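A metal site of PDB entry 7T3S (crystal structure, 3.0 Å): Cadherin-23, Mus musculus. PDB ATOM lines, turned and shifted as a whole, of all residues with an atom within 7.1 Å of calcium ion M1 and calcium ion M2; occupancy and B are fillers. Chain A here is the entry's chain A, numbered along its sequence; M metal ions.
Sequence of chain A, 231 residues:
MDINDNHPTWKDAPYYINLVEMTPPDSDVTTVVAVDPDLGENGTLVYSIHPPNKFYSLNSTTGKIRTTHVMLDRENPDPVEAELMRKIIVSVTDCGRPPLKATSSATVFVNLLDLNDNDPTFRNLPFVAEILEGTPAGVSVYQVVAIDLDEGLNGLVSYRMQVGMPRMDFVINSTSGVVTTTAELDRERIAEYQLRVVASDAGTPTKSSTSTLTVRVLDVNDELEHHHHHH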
ATOM      1  N   GLU A  21     -34.253 -23.331 -11.228  1.00  0.00           N
ATOM      2  CA  GLU A  21     -34.950 -24.611 -10.950  1.00  0.00           C
ATOM      3  C   GLU A  21     -35.648 -24.489  -9.601  1.00  0.00           C
ATOM      4  O   GLU A  21     -35.241 -23.631  -8.819  1.00  0.00           O
ATOM      5  CB  GLU A  21     -33.961 -25.789 -10.971  1.00  0.00           C
ATOM      6  CG  GLU A  21     -33.016 -25.844  -9.785  1.00  0.00           C
ATOM      7  CD  GLU A  21     -32.130 -27.055  -9.761  1.00  0.00           C
ATOM      8  OE1 GLU A  21     -32.659 -28.191 -10.024  1.00  0.00           O
ATOM      9  OE2 GLU A  21     -30.903 -26.900  -9.473  1.00  0.00           O
ATOM     10  N   MET A  22     -36.674 -25.318  -9.374  1.00  0.00           N
ATOM     11  CA  MET A  22     -37.512 -25.344  -8.139  1.00  0.00           C
ATOM     12  C   MET A  22     -38.335 -24.039  -8.016  1.00  0.00           C
ATOM     13  O   MET A  22     -39.050 -23.880  -7.000  1.00  0.00           O
ATOM     14  CB  MET A  22     -36.662 -25.557  -6.861  1.00  0.00           C
ATOM     15  CG  MET A  22     -35.875 -26.868  -6.853  1.00  0.00           C
ATOM     16  SD  MET A  22     -36.964 -28.336  -6.890  1.00  0.00           S
ATOM     17  CE  MET A  22     -35.791 -29.654  -7.189  1.00  0.00           C
ATOM     18  N   ASP A  73     -36.620 -29.540 -12.031  1.00  0.00           N
ATOM     19  CA  ASP A  73     -35.436 -30.191 -11.421  1.00  0.00           C
ATOM     20  C   ASP A  73     -34.354 -30.312 -12.496  1.00  0.00           C
ATOM     21  O   ASP A  73     -34.574 -31.075 -13.455  1.00  0.00           O
ATOM     22  CB  ASP A  73     -35.860 -31.533 -10.812  1.00  0.00           C
ATOM     23  CG  ASP A  73     -34.788 -32.248 -10.007  1.00  0.00           C
ATOM     24  OD1 ASP A  73     -33.629 -31.745  -9.965  1.00  0.00           O
ATOM     25  OD2 ASP A  73     -35.122 -33.286  -9.419  1.00  0.00           O
ATOM     26  N   ARG A  74     -33.217 -29.592 -12.357  1.00  0.00           N
ATOM     27  CA  ARG A  74     -32.102 -29.570 -13.374  1.00  0.00           C
ATOM     28  C   ARG A  74     -31.435 -30.955 -13.438  1.00  0.00           C
ATOM     29  O   ARG A  74     -30.948 -31.308 -14.509  1.00  0.00           O
ATOM     30  CB  ARG A  74     -31.058 -28.493 -13.043  1.00  0.00           C
ATOM     31  CG  ARG A  74     -30.211 -28.066 -14.247  1.00  0.00           C
ATOM     32  CD  ARG A  74     -28.887 -27.404 -13.863  1.00  0.00           C
ATOM     33  NE  ARG A  74     -28.023 -28.341 -13.165  1.00  0.00           N
ATOM     34  CZ  ARG A  74     -27.329 -29.358 -13.734  1.00  0.00           C
ATOM     35  NH1 ARG A  74     -26.582 -30.156 -12.976  1.00  0.00           N
ATOM     36  NH2 ARG A  74     -27.378 -29.577 -15.051  1.00  0.00           N
ATOM     37  N   GLU A  75     -31.447 -31.682 -12.323  1.00  0.00           N
ATOM     38  CA  GLU A  75     -30.833 -33.026 -12.169  1.00  0.00           C
ATOM     39  C   GLU A  75     -31.872 -34.151 -12.422  1.00  0.00           C
ATOM     40  O   GLU A  75     -31.544 -35.317 -12.097  1.00  0.00           O
ATOM     41  CB  GLU A  75     -30.190 -33.135 -10.779  1.00  0.00           C
ATOM     42  CG  GLU A  75     -28.957 -32.238 -10.592  1.00  0.00           C
ATOM     43  CD  GLU A  75     -29.202 -30.743 -10.428  1.00  0.00           C
ATOM     44  OE1 GLU A  75     -30.122 -30.382  -9.677  1.00  0.00           O
ATOM     45  OE2 GLU A  75     -28.470 -29.957 -11.022  1.00  0.00           O
ATOM     46  N   LEU A 113     -31.414 -22.684 -14.615  1.00  0.00           N
ATOM     47  CA  LEU A 113     -30.285 -22.268 -13.767  1.00  0.00           C
ATOM     48  C   LEU A 113     -30.275 -23.168 -12.530  1.00  0.00           C
ATOM     49  O   LEU A 113     -31.357 -23.546 -12.060  1.00  0.00           O
ATOM     50  CB  LEU A 113     -30.419 -20.788 -13.421  1.00  0.00           C
ATOM     51  CG  LEU A 113     -30.284 -19.856 -14.622  1.00  0.00           C
ATOM     52  CD1 LEU A 113     -30.671 -18.432 -14.252  1.00  0.00           C
ATOM     53  CD2 LEU A 113     -28.866 -19.918 -15.193  1.00  0.00           C
ATOM     54  N   ASP A 114     -29.067 -23.488 -12.063  1.00  0.00           N
ATOM     55  CA  ASP A 114     -28.783 -24.511 -11.040  1.00  0.00           C
ATOM     56  C   ASP A 114     -28.828 -23.894  -9.654  1.00  0.00           C
ATOM     57  O   ASP A 114     -28.341 -22.807  -9.488  1.00  0.00           O
ATOM     58  CB  ASP A 114     -27.396 -25.121 -11.253  1.00  0.00           C
ATOM     59  CG  ASP A 114     -27.076 -26.244 -10.287  1.00  0.00           C
ATOM     60  OD1 ASP A 114     -27.887 -27.206 -10.199  1.00  0.00           O
ATOM     61  OD2 ASP A 114     -26.036 -26.157  -9.636  1.00  0.00           O
ATOM     62  N   LEU A 115     -29.414 -24.609  -8.720  1.00  0.00           N
ATOM     63  CA  LEU A 115     -29.324 -24.353  -7.275  1.00  0.00           C
ATOM     64  C   LEU A 115     -28.492 -25.461  -6.681  1.00  0.00           C
ATOM     65  O   LEU A 115     -28.485 -26.546  -7.268  1.00  0.00           O
ATOM     66  CB  LEU A 115     -30.724 -24.348  -6.642  1.00  0.00           C
ATOM     67  CG  LEU A 115     -31.636 -23.189  -7.006  1.00  0.00           C
ATOM     68  CD1 LEU A 115     -32.941 -23.295  -6.217  1.00  0.00           C
ATOM     69  CD2 LEU A 115     -30.961 -21.845  -6.764  1.00  0.00           C
ATOM     70  N   ASN A 116     -27.849 -25.197  -5.561  1.00  0.00           N
ATOM     71  CA  ASN A 116     -27.135 -26.217  -4.762  1.00  0.00           C
ATOM     72  C   ASN A 116     -28.201 -26.964  -3.953  1.00  0.00           C
ATOM     73  O   ASN A 116     -28.150 -26.899  -2.741  1.00  0.00           O
ATOM     74  CB  ASN A 116     -26.029 -25.588  -3.903  1.00  0.00           C
ATOM     75  CG  ASN A 116     -25.013 -26.596  -3.410  1.00  0.00           C
ATOM     76  OD1 ASN A 116     -24.968 -27.736  -3.857  1.00  0.00           O
ATOM     77  ND2 ASN A 116     -24.183 -26.187  -2.472  1.00  0.00           N
ATOM     78  N   ASP A 117     -29.112 -27.637  -4.633  1.00  0.00           N
ATOM     79  CA  ASP A 117     -30.293 -28.278  -4.005  1.00  0.00           C
ATOM     80  C   ASP A 117     -29.980 -29.755  -3.688  1.00  0.00           C
ATOM     81  O   ASP A 117     -30.723 -30.346  -2.853  1.00  0.00           O
ATOM     82  CB  ASP A 117     -31.547 -28.084  -4.876  1.00  0.00           C
ATOM     83  CG  ASP A 117     -31.537 -28.834  -6.189  1.00  0.00           C
ATOM     84  OD1 ASP A 117     -30.423 -29.068  -6.741  1.00  0.00           O
ATOM     85  OD2 ASP A 117     -32.653 -29.187  -6.681  1.00  0.00           O
ATOM     86  N   ASN A 118     -28.937 -30.339  -4.327  1.00  0.00           N
ATOM     87  CA  ASN A 118     -28.458 -31.717  -4.072  1.00  0.00           C
ATOM     88  C   ASN A 118     -27.198 -31.690  -3.199  1.00  0.00           C
ATOM     89  O   ASN A 118     -26.399 -30.735  -3.316  1.00  0.00           O
ATOM     90  CB  ASN A 118     -28.184 -32.475  -5.367  1.00  0.00           C
ATOM     91  CG  ASN A 118     -29.435 -32.814  -6.128  1.00  0.00           C
ATOM     92  OD1 ASN A 118     -30.477 -32.177  -5.945  1.00  0.00           O
ATOM     93  ND2 ASN A 118     -29.356 -33.806  -6.990  1.00  0.00           N
ATOM     94  N   ASP A 119     -27.046 -32.716  -2.352  1.00  0.00           N
ATOM     95  CA  ASP A 119     -25.885 -32.962  -1.462  1.00  0.00           C
ATOM     96  C   ASP A 119     -25.030 -34.073  -2.070  1.00  0.00           C
ATOM     97  O   ASP A 119     -25.492 -34.795  -2.966  1.00  0.00           O
ATOM     98  CB  ASP A 119     -26.334 -33.296  -0.021  1.00  0.00           C
ATOM     99  CG  ASP A 119     -27.465 -34.317   0.083  1.00  0.00           C
ATOM    100  OD1 ASP A 119     -27.483 -35.292  -0.729  1.00  0.00           O
ATOM    101  OD2 ASP A 119     -28.337 -34.142   0.967  1.00  0.00           O
ATOM    102  N   PRO A 120     -23.750 -34.257  -1.636  1.00  0.00           N
ATOM    103  CA  PRO A 120     -22.947 -35.361  -2.127  1.00  0.00           C
ATOM    104  C   PRO A 120     -23.550 -36.704  -1.677  1.00  0.00           C
ATOM    105  O   PRO A 120     -24.120 -36.757  -0.577  1.00  0.00           O
ATOM    106  CB  PRO A 120     -21.549 -35.118  -1.496  1.00  0.00           C
ATOM    107  CG  PRO A 120     -21.575 -33.656  -1.063  1.00  0.00           C
ATOM    108  CD  PRO A 120     -23.009 -33.406  -0.679  1.00  0.00           C
ATOM    109  N   ASP A 148     -21.826 -35.543  -6.756  1.00  0.00           N
ATOM    110  CA  ASP A 148     -22.855 -34.507  -6.532  1.00  0.00           C
ATOM    111  C   ASP A 148     -23.401 -34.126  -7.917  1.00  0.00           C
ATOM    112  O   ASP A 148     -22.588 -33.662  -8.771  1.00  0.00           O
ATOM    113  CB  ASP A 148     -22.269 -33.357  -5.731  1.00  0.00           C
ATOM    114  CG  ASP A 148     -23.264 -32.288  -5.312  1.00  0.00           C
ATOM    115  OD1 ASP A 148     -24.213 -32.013  -6.074  1.00  0.00           O
ATOM    116  OD2 ASP A 148     -23.084 -31.733  -4.221  1.00  0.00           O
ATOM    117  N   LEU A 149     -24.715 -34.299  -8.120  1.00  0.00           N
ATOM    118  CA  LEU A 149     -25.385 -34.171  -9.444  1.00  0.00           C
ATOM    119  C   LEU A 149     -25.513 -32.706  -9.864  1.00  0.00           C
ATOM    120  O   LEU A 149     -25.805 -32.457 -11.037  1.00  0.00           O
ATOM    121  CB  LEU A 149     -26.771 -34.831  -9.375  1.00  0.00           C
ATOM    122  CG  LEU A 149     -26.782 -36.335  -9.058  1.00  0.00           C
ATOM    123  CD1 LEU A 149     -28.204 -36.855  -8.916  1.00  0.00           C
ATOM    124  CD2 LEU A 149     -26.015 -37.131 -10.123  1.00  0.00           C
ATOM    125  N   ASP A 150     -25.302 -31.768  -8.935  1.00  0.00           N
ATOM    126  CA  ASP A 150     -25.323 -30.314  -9.214  1.00  0.00           C
ATOM    127  C   ASP A 150     -24.209 -29.950 -10.213  1.00  0.00           C
ATOM    128  O   ASP A 150     -23.340 -30.815 -10.497  1.00  0.00           O
ATOM    129  CB  ASP A 150     -25.222 -29.483  -7.933  1.00  0.00           C
ATOM    130  CG  ASP A 150     -26.440 -29.566  -7.035  1.00  0.00           C
ATOM    131  OD1 ASP A 150     -27.555 -29.837  -7.539  1.00  0.00           O
ATOM    132  OD2 ASP A 150     -26.261 -29.350  -5.853  1.00  0.00           O
ATOM    133  N   GLU A 151     -24.263 -28.708 -10.707  1.00  0.00           N
ATOM    134  CA  GLU A 151     -23.430 -28.147 -11.805  1.00  0.00           C
ATOM    135  C   GLU A 151     -22.268 -27.342 -11.226  1.00  0.00           C
ATOM    136  O   GLU A 151     -22.429 -26.762 -10.134  1.00  0.00           O
ATOM    137  CB  GLU A 151     -24.332 -27.264 -12.677  1.00  0.00           C
ATOM    138  CG  GLU A 151     -23.718 -26.777 -13.969  1.00  0.00           C
ATOM    139  CD  GLU A 151     -24.716 -26.043 -14.865  1.00  0.00           C
ATOM    140  OE1 GLU A 151     -25.839 -26.587 -15.085  1.00  0.00           O
ATOM    141  OE2 GLU A 151     -24.379 -24.933 -15.349  1.00  0.00           O
ATOM    142  N   LEU A 153     -19.217 -25.690  -9.466  1.00  0.00           N
ATOM    143  CA  LEU A 153     -18.696 -25.716  -8.075  1.00  0.00           C
ATOM    144  C   LEU A 153     -19.677 -26.460  -7.158  1.00  0.00           C
ATOM    145  O   LEU A 153     -19.211 -27.139  -6.260  1.00  0.00           O
ATOM    146  CB  LEU A 153     -18.456 -24.285  -7.585  1.00  0.00           C
ATOM    147  CG  LEU A 153     -17.336 -23.509  -8.314  1.00  0.00           C
ATOM    148  CD1 LEU A 153     -17.336 -22.059  -7.892  1.00  0.00           C
ATOM    149  CD2 LEU A 153     -15.966 -24.142  -8.062  1.00  0.00           C
ATOM    150  N   ASN A 154     -20.988 -26.358  -7.406  1.00  0.00           N
ATOM    151  CA  ASN A 154     -22.058 -26.996  -6.572  1.00  0.00           C
ATOM    152  C   ASN A 154     -21.955 -28.534  -6.624  1.00  0.00           C
ATOM    153  O   ASN A 154     -22.492 -29.162  -5.720  1.00  0.00           O
ATOM    154  CB  ASN A 154     -23.462 -26.569  -6.986  1.00  0.00           C
ATOM    155  CG  ASN A 154     -23.756 -25.109  -6.689  1.00  0.00           C
ATOM    156  OD1 ASN A 154     -23.445 -24.617  -5.611  1.00  0.00           O
ATOM    157  ND2 ASN A 154     -24.357 -24.433  -7.632  1.00  0.00           N
ATOM    158  N   GLY A 155     -21.316 -29.108  -7.648  1.00  0.00           N
ATOM    159  CA  GLY A 155     -21.151 -30.563  -7.832  1.00  0.00           C
ATOM    160  C   GLY A 155     -19.749 -31.044  -7.499  1.00  0.00           C
ATOM    161  O   GLY A 155     -19.545 -32.259  -7.573  1.00  0.00           O
ATOM    162  N   LEU A 156     -18.836 -30.146  -7.138  1.00  0.00           N
ATOM    163  CA  LEU A 156     -17.399 -30.482  -6.910  1.00  0.00           C
ATOM    164  C   LEU A 156     -17.216 -30.982  -5.467  1.00  0.00           C
ATOM    165  O   LEU A 156     -17.205 -30.135  -4.538  1.00  0.00           O
ATOM    166  CB  LEU A 156     -16.546 -29.246  -7.219  1.00  0.00           C
ATOM    167  CG  LEU A 156     -15.055 -29.355  -6.867  1.00  0.00           C
ATOM    168  CD1 LEU A 156     -14.430 -30.617  -7.427  1.00  0.00           C
ATOM    169  CD2 LEU A 156     -14.300 -28.127  -7.344  1.00  0.00           C
ATOM    170  N   ASP A 201     -19.404 -30.192  -0.884  1.00  0.00           N
ATOM    171  CA  ASP A 201     -19.331 -29.584  -2.239  1.00  0.00           C
ATOM    172  C   ASP A 201     -18.765 -28.184  -2.067  1.00  0.00           C
ATOM    173  O   ASP A 201     -18.387 -27.862  -0.948  1.00  0.00           O
ATOM    174  CB  ASP A 201     -20.688 -29.635  -2.939  1.00  0.00           C
ATOM    175  CG  ASP A 201     -21.820 -28.937  -2.220  1.00  0.00           C
ATOM    176  OD1 ASP A 201     -21.547 -28.072  -1.365  1.00  0.00           O
ATOM    177  OD2 ASP A 201     -22.969 -29.251  -2.523  1.00  0.00           O
ATOM    178  N   ALA A 202     -18.711 -27.383  -3.146  1.00  0.00           N
ATOM    179  CA  ALA A 202     -18.088 -26.035  -3.152  1.00  0.00           C
ATOM    180  C   ALA A 202     -19.149 -24.909  -3.282  1.00  0.00           C
ATOM    181  O   ALA A 202     -18.780 -23.804  -3.735  1.00  0.00           O
ATOM    182  CB  ALA A 202     -17.059 -25.967  -4.261  1.00  0.00           C
ATOM    183  N   GLY A 203     -20.416 -25.150  -2.898  1.00  0.00           N
ATOM    184  CA  GLY A 203     -21.456 -24.108  -2.873  1.00  0.00           C
ATOM    185  C   GLY A 203     -21.223 -23.139  -1.724  1.00  0.00           C
ATOM    186  O   GLY A 203     -20.622 -23.558  -0.718  1.00  0.00           O
ATOM    187  N   PRO A 205     -23.484 -21.851   0.334  1.00  0.00           N
ATOM    188  CA  PRO A 205     -24.062 -22.543   1.481  1.00  0.00           C
ATOM    189  C   PRO A 205     -23.720 -24.045   1.291  1.00  0.00           C
ATOM    190  O   PRO A 205     -24.518 -24.778   0.723  1.00  0.00           O
ATOM    191  CB  PRO A 205     -25.546 -22.207   1.324  1.00  0.00           C
ATOM    192  CG  PRO A 205     -25.744 -22.061  -0.228  1.00  0.00           C
ATOM    193  CD  PRO A 205     -24.344 -21.998  -0.843  1.00  0.00           C
ATOM    194  N   LYS A 207     -23.062 -27.952   1.268  1.00  0.00           N
ATOM    195  CA  LYS A 207     -23.890 -29.142   1.605  1.00  0.00           C
ATOM    196  C   LYS A 207     -22.960 -30.340   1.797  1.00  0.00           C
ATOM    197  O   LYS A 207     -22.072 -30.548   0.935  1.00  0.00           O
ATOM    198  CB  LYS A 207     -24.926 -29.409   0.524  1.00  0.00           C
ATOM    199  CG  LYS A 207     -25.950 -28.313   0.356  1.00  0.00           C
ATOM    200  CD  LYS A 207     -27.247 -28.760  -0.251  1.00  0.00           C
ATOM    201  CE  LYS A 207     -28.059 -29.644   0.684  1.00  0.00           C
ATOM    202  NZ  LYS A 207     -29.369 -30.009   0.082  1.00  0.00           N
HETATM  203 CA    CA M   1     -24.467 -29.784  -4.255  1.00  0.00          CA
HETATM  204 CA    CA M   2     -29.246 -28.253  -8.615  1.00  0.00          CA
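Six residues have an atom within 4 Å of calcium ion M2: Glu 21, Glu 75, Asp 114, Leu 115, Asp 117 and Asp 150.
The nearest printed residue that does not touch calcium ion M2 is Asn 116 (4.5 Å).
O of Leu 115 binds calcium ion M2.
The side-chain carboxylate (OE2) of Glu 21 is bound to calcium ion M2.
OD1 of Asp 114 binds calcium ion M2 (2.3 Å).
The side-chain carboxylate (OD1) of Asp 117 is bound to calcium ion M2, 2.4 Å away.
OE1 of Glu 75 binds calcium ion M2 (2.5 Å).
Calcium ion M2 is bound by OD1 of Asp 150 (2.6 Å).
Slightly farther from calcium ion M2 lies the side-chain carboxylate (OE2) of Glu 75 (3.0 Å).
The side-chain carboxylate (OE1) of Glu 21 sits at hydrogen-bond distance from the backbone NH (N) of Arg 74 (2.8 Å).
The backbone NH (N) of Glu 21 sits at hydrogen-bond distance from the backbone carbonyl oxygen (O) of Leu 113, 3.0 Å away.
The side-chain amide nitrogen (ND2) of Asn 154 is in hydrogen-bond range of the side-chain carboxylate (OD2) of Asp 114, at 3.1 Å.
The backbone NH (N) of Glu 151 lies within hydrogen-bond range of the side-chain carboxylate (OD2) of Asp 114 (3.3 Å).
The side-chain amide oxygen (OD1) of Asn 118 lies close to the side-chain carboxylate (OD1) of Asp 117.
The backbone NH of Gly 203 is in hydrogen-bond range of the side-chain carboxylate of Asp 201, at 3.5 Å.
NZ of Lys 207 lies within hydrogen-bond range of O of Asp 117.
The side-chain carboxylate (OE2) of Glu 75 is in salt-bridge range of the guanidinium group (NE) of Arg 74.
Calcium ion M1 is bound by the side-chain amide oxygen (OD1) of Asn 116 (2.1 Å), the backbone carbonyl oxygen (O) of Asn 118 (2.3 Å), the side-chain carboxylate (OD2) of Asp 201 (2.4 Å), the side-chain carboxylate (OD2) of Asp 148 (2.4 Å), the side-chain carboxylate (OD2) of Asp 150 (2.4 Å), the backbone carbonyl oxygen (O) of Asn 154 (2.5 Å) and the side-chain carboxylate (OD1) of Asp 148 (2.9 Å).
Calcium ion M1 has seven donor atoms within binding distance.
Within 4 Å of calcium ion M1: Asn 116, Asn 118, Asp 148, Asp 150, Asn 154 and Asp 201.
The nearest printed residue that does not touch calcium ion M1 is Asp 119 (4.3 Å).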
